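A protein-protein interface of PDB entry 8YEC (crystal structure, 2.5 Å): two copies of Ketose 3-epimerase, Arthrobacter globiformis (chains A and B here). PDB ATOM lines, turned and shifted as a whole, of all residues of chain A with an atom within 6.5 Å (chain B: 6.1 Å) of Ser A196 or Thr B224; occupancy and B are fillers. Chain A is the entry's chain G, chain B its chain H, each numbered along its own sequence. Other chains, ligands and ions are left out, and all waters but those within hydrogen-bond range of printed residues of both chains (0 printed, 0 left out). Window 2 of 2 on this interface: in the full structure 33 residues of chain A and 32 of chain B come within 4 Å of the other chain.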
ATOM      1  N   MET A 191      11.606  22.891  18.600  1.00  0.00           N
ATOM      2  CA  MET A 191      11.221  21.999  17.517  1.00  0.00           C
ATOM      3  C   MET A 191      12.054  22.320  16.284  1.00  0.00           C
ATOM      4  O   MET A 191      12.421  21.421  15.542  1.00  0.00           O
ATOM      5  CB  MET A 191       9.747  22.145  17.139  1.00  0.00           C
ATOM      6  CG  MET A 191       8.826  21.167  17.825  1.00  0.00           C
ATOM      7  SD  MET A 191       7.158  21.862  17.902  1.00  0.00           S
ATOM      8  CE  MET A 191       6.524  21.234  16.346  1.00  0.00           C
ATOM      9  N   ILE A 193      14.922  22.883  15.910  1.00  0.00           N
ATOM     10  CA  ILE A 193      16.230  22.260  15.915  1.00  0.00           C
ATOM     11  C   ILE A 193      16.074  20.749  15.784  1.00  0.00           C
ATOM     12  O   ILE A 193      16.540  20.162  14.812  1.00  0.00           O
ATOM     13  CB  ILE A 193      17.026  22.691  17.161  1.00  0.00           C
ATOM     14  CG1 ILE A 193      17.149  24.215  17.215  1.00  0.00           C
ATOM     15  CG2 ILE A 193      18.380  22.027  17.147  1.00  0.00           C
ATOM     16  CD1 ILE A 193      17.717  24.786  18.482  1.00  0.00           C
ATOM     17  N   GLU A 194      15.373  20.116  16.726  1.00  0.00           N
ATOM     18  CA  GLU A 194      15.513  18.677  16.930  1.00  0.00           C
ATOM     19  C   GLU A 194      14.595  17.824  16.035  1.00  0.00           C
ATOM     20  O   GLU A 194      14.966  16.706  15.672  1.00  0.00           O
ATOM     21  CB  GLU A 194      15.266  18.345  18.403  1.00  0.00           C
ATOM     22  CG  GLU A 194      16.254  19.018  19.362  1.00  0.00           C
ATOM     23  CD  GLU A 194      17.700  18.591  19.176  1.00  0.00           C
ATOM     24  OE1 GLU A 194      17.915  17.522  18.596  1.00  0.00           O
ATOM     25  OE2 GLU A 194      18.610  19.329  19.590  1.00  0.00           O
ATOM     26  N   GLU A 195      13.402  18.309  15.681  1.00  0.00           N
ATOM     27  CA  GLU A 195      12.388  17.462  15.070  1.00  0.00           C
ATOM     28  C   GLU A 195      12.604  17.312  13.556  1.00  0.00           C
ATOM     29  O   GLU A 195      13.335  18.089  12.919  1.00  0.00           O
ATOM     30  CB  GLU A 195      11.008  18.055  15.350  1.00  0.00           C
ATOM     31  CG  GLU A 195      10.750  18.343  16.813  1.00  0.00           C
ATOM     32  CD  GLU A 195      10.455  17.105  17.641  1.00  0.00           C
ATOM     33  OE1 GLU A 195      10.374  16.001  17.040  1.00  0.00           O
ATOM     34  OE2 GLU A 195      10.299  17.246  18.890  1.00  0.00           O
ATOM     35  N   SER A 196      11.909  16.311  12.985  1.00  0.00           N
ATOM     36  CA  SER A 196      11.988  15.965  11.570  1.00  0.00           C
ATOM     37  C   SER A 196      11.233  16.957  10.685  1.00  0.00           C
ATOM     38  O   SER A 196      11.504  16.993   9.486  1.00  0.00           O
ATOM     39  CB  SER A 196      11.455  14.590  11.317  1.00  0.00           C
ATOM     40  OG  SER A 196      10.031  14.621  11.271  1.00  0.00           O
ATOM     41  N   ASP A 197      10.266  17.689  11.271  1.00  0.00           N
ATOM     42  CA  ASP A 197       9.411  18.664  10.598  1.00  0.00           C
ATOM     43  C   ASP A 197       8.453  19.243  11.637  1.00  0.00           C
ATOM     44  O   ASP A 197       8.546  18.881  12.796  1.00  0.00           O
ATOM     45  CB  ASP A 197       8.647  18.042   9.426  1.00  0.00           C
ATOM     46  CG  ASP A 197       7.766  16.894   9.859  1.00  0.00           C
ATOM     47  OD1 ASP A 197       6.702  17.185  10.445  1.00  0.00           O
ATOM     48  OD2 ASP A 197       8.178  15.721   9.652  1.00  0.00           O
ATOM     49  N   MET A 198       7.530  20.129  11.240  1.00  0.00           N
ATOM     50  CA  MET A 198       6.690  20.829  12.202  1.00  0.00           C
ATOM     51  C   MET A 198       5.301  20.196  12.319  1.00  0.00           C
ATOM     52  O   MET A 198       4.477  20.704  13.072  1.00  0.00           O
ATOM     53  CB  MET A 198       6.493  22.302  11.822  1.00  0.00           C
ATOM     54  CG  MET A 198       7.733  23.163  11.899  1.00  0.00           C
ATOM     55  SD  MET A 198       8.683  22.894  13.407  1.00  0.00           S
ATOM     56  CE  MET A 198       8.050  24.218  14.438  1.00  0.00           C
ATOM     57  N   SER A 200       4.695  16.324  12.019  1.00  0.00           N
ATOM     58  CA  SER A 200       4.800  14.993  12.600  1.00  0.00           C
ATOM     59  C   SER A 200       4.814  15.024  14.129  1.00  0.00           C
ATOM     60  O   SER A 200       4.100  14.231  14.740  1.00  0.00           O
ATOM     61  CB  SER A 200       6.020  14.278  12.075  1.00  0.00           C
ATOM     62  OG  SER A 200       5.999  14.238  10.658  1.00  0.00           O
ATOM     63  N   PRO A 201       5.627  15.872  14.816  1.00  0.00           N
ATOM     64  CA  PRO A 201       5.557  15.933  16.274  1.00  0.00           C
ATOM     65  C   PRO A 201       4.158  16.221  16.813  1.00  0.00           C
ATOM     66  O   PRO A 201       3.801  15.640  17.827  1.00  0.00           O
ATOM     67  CB  PRO A 201       6.527  17.053  16.648  1.00  0.00           C
ATOM     68  CG  PRO A 201       7.491  17.110  15.484  1.00  0.00           C
ATOM     69  CD  PRO A 201       6.635  16.810  14.275  1.00  0.00           C
ATOM     70  N   GLU B 216      21.867  19.686   8.479  1.00  0.00           N
ATOM     71  CA  GLU B 216      20.445  19.719   8.773  1.00  0.00           C
ATOM     72  C   GLU B 216      20.215  20.344  10.152  1.00  0.00           C
ATOM     73  O   GLU B 216      21.132  20.465  10.970  1.00  0.00           O
ATOM     74  CB  GLU B 216      19.883  18.297   8.692  1.00  0.00           C
ATOM     75  CG  GLU B 216      18.374  18.212   8.768  1.00  0.00           C
ATOM     76  CD  GLU B 216      17.691  19.107   7.749  1.00  0.00           C
ATOM     77  OE1 GLU B 216      17.480  18.625   6.618  1.00  0.00           O
ATOM     78  OE2 GLU B 216      17.401  20.301   8.080  1.00  0.00           O
ATOM     79  N   SER B 217      18.962  20.726  10.419  1.00  0.00           N
ATOM     80  CA  SER B 217      18.588  21.390  11.662  1.00  0.00           C
ATOM     81  C   SER B 217      18.963  20.556  12.893  1.00  0.00           C
ATOM     82  O   SER B 217      19.306  21.127  13.928  1.00  0.00           O
ATOM     83  CB  SER B 217      17.121  21.726  11.667  1.00  0.00           C
ATOM     84  OG  SER B 217      16.342  20.543  11.584  1.00  0.00           O
ATOM     85  N   HIS B 218      18.873  19.219  12.787  1.00  0.00           N
ATOM     86  CA  HIS B 218      19.273  18.323  13.860  1.00  0.00           C
ATOM     87  C   HIS B 218      20.638  17.671  13.610  1.00  0.00           C
ATOM     88  O   HIS B 218      21.066  16.848  14.418  1.00  0.00           O
ATOM     89  CB  HIS B 218      18.214  17.236  14.082  1.00  0.00           C
ATOM     90  CG  HIS B 218      17.758  16.572  12.822  1.00  0.00           C
ATOM     91  ND1 HIS B 218      18.635  16.091  11.881  1.00  0.00           N
ATOM     92  CD2 HIS B 218      16.539  16.350  12.334  1.00  0.00           C
ATOM     93  CE1 HIS B 218      17.958  15.590  10.870  1.00  0.00           C
ATOM     94  NE2 HIS B 218      16.680  15.740  11.119  1.00  0.00           N
ATOM     95  N   GLY B 220      21.510  15.606  11.193  1.00  0.00           N
ATOM     96  CA  GLY B 220      21.382  14.265  10.636  1.00  0.00           C
ATOM     97  C   GLY B 220      21.307  14.297   9.111  1.00  0.00           C
ATOM     98  O   GLY B 220      21.961  15.125   8.480  1.00  0.00           O
ATOM     99  N   TYR B 221      20.501  13.392   8.532  1.00  0.00           N
ATOM    100  CA  TYR B 221      20.336  13.318   7.090  1.00  0.00           C
ATOM    101  C   TYR B 221      19.906  14.653   6.487  1.00  0.00           C
ATOM    102  O   TYR B 221      19.054  15.351   7.038  1.00  0.00           O
ATOM    103  CB  TYR B 221      19.269  12.296   6.708  1.00  0.00           C
ATOM    104  CG  TYR B 221      19.801  10.914   6.479  1.00  0.00           C
ATOM    105  CD1 TYR B 221      19.961  10.019   7.522  1.00  0.00           C
ATOM    106  CD2 TYR B 221      20.176  10.508   5.206  1.00  0.00           C
ATOM    107  CE1 TYR B 221      20.457   8.738   7.300  1.00  0.00           C
ATOM    108  CE2 TYR B 221      20.678   9.235   4.968  1.00  0.00           C
ATOM    109  CZ  TYR B 221      20.822   8.347   6.019  1.00  0.00           C
ATOM    110  OH  TYR B 221      21.314   7.087   5.782  1.00  0.00           O
ATOM    111  N   LEU B 222      20.469  14.990   5.321  1.00  0.00           N
ATOM    112  CA  LEU B 222      20.096  16.231   4.658  1.00  0.00           C
ATOM    113  C   LEU B 222      18.679  16.114   4.108  1.00  0.00           C
ATOM    114  O   LEU B 222      18.314  15.123   3.485  1.00  0.00           O
ATOM    115  CB  LEU B 222      21.119  16.578   3.574  1.00  0.00           C
ATOM    116  CG  LEU B 222      22.535  16.864   4.086  1.00  0.00           C
ATOM    117  CD1 LEU B 222      23.378  17.447   2.979  1.00  0.00           C
ATOM    118  CD2 LEU B 222      22.536  17.823   5.281  1.00  0.00           C
ATOM    119  N   GLY B 223      17.870  17.140   4.384  1.00  0.00           N
ATOM    120  CA  GLY B 223      16.473  17.152   3.977  1.00  0.00           C
ATOM    121  C   GLY B 223      15.537  16.342   4.881  1.00  0.00           C
ATOM    122  O   GLY B 223      14.447  16.002   4.432  1.00  0.00           O
ATOM    123  N   THR B 224      15.931  16.043   6.135  1.00  0.00           N
ATOM    124  CA  THR B 224      15.021  15.415   7.097  1.00  0.00           C
ATOM    125  C   THR B 224      14.735  16.302   8.317  1.00  0.00           C
ATOM    126  O   THR B 224      14.374  15.805   9.380  1.00  0.00           O
ATOM    127  CB  THR B 224      15.545  14.056   7.575  1.00  0.00           C
ATOM    128  OG1 THR B 224      16.754  14.229   8.314  1.00  0.00           O
ATOM    129  CG2 THR B 224      15.781  13.104   6.429  1.00  0.00           C
ATOM    130  N   GLY B 225      14.875  17.621   8.172  1.00  0.00           N
ATOM    131  CA  GLY B 225      14.751  18.531   9.298  1.00  0.00           C
ATOM    132  C   GLY B 225      14.144  19.838   8.829  1.00  0.00           C
ATOM    133  O   GLY B 225      13.367  19.840   7.891  1.00  0.00           O
ATOM    134  N   SER B 226      14.557  20.941   9.444  1.00  0.00           N
ATOM    135  CA  SER B 226      13.868  22.211   9.278  1.00  0.00           C
ATOM    136  C   SER B 226      14.718  23.274   8.571  1.00  0.00           C
ATOM    137  O   SER B 226      14.378  24.448   8.628  1.00  0.00           O
ATOM    138  CB  SER B 226      13.395  22.712  10.637  1.00  0.00           C
ATOM    139  OG  SER B 226      12.218  22.026  11.065  1.00  0.00           O
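No position is printed for both chains. Of the 7 pairs that touch across the chains among the printed residues, none has its exchanged pair printed and touching as well.
O of Glu A194 touches CB of His B218, at 3.7 Å. Glu A195 touches His B218. O of Glu A195 touches CA of Gly B225, at 3.9 Å. Gly B225 touches Ser A196 (CA to O, 3.6 Å).
O of Thr B224 lies within hydrogen-bond range of NE2 of His B218 (2.9 Å). The side-chain carboxylate (OD2) of Asp A197 lies within hydrogen-bond range of the side-chain hydroxyl (OG) of Ser A196, at 2.7 Å. The backbone carbonyl oxygen (O) of Tyr B221 is in hydrogen-bond range of the side-chain hydroxyl (OG1) of Thr B224 (2.9 Å). The backbone NH (N) of Ser B226 is in hydrogen-bond range of the side-chain hydroxyl (OG) of Ser B217 (2.8 Å). OE1 of Glu B216 sits at hydrogen-bond distance from N of Gly B225, at 3.2 Å. N of Thr B224 is in hydrogen-bond range of OE1 of Glu B216.
Of chain B, only Thr B224 (3.1 Å) and Gly B225 (3.6 Å) come within 4 Å of Ser A196. Thr B224 touches just one residue of chain A: Ser A196 (3.1 Å). Printed residues of chain A within 4 Å of Ser B217: Ile A193. Printed residues of chain A within 4 Å of His B218: Ile A193 (3.2 Å), Glu A194 (3.7 Å) and Glu A195 (3.7 Å). Of the printed residues of chain B, Ile A193 touches Ser B217 and His B218. Ser B226 touches none of the printed residues of chain A.
The backbone carbonyl oxygen (O) of Thr B224 lies close to the backbone carbonyl oxygen (O) of Ser A196, at 3.1 Å. The backbone carbonyl oxygen (O) of Ile A193 sits close to the side-chain hydroxyl (OG) of Ser B217, at 3.3 Å. O of Ile A193 lies within hydrogen-bond range of N of His B218 (3.2 Å).
Printed residues of chain A that touch a printed residue of chain B: Ile A193, Glu A194, Glu A195 and Ser A196. Printed residues of chain B that touch a printed residue of chain A: Ser B217, His B218, Thr B224 and Gly B225. Hydrophobic or aromatic side chains of chain B within 4 Å of the printed part of chain A: His B218. Among the printed residues, 7 pairs touch across the chains.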
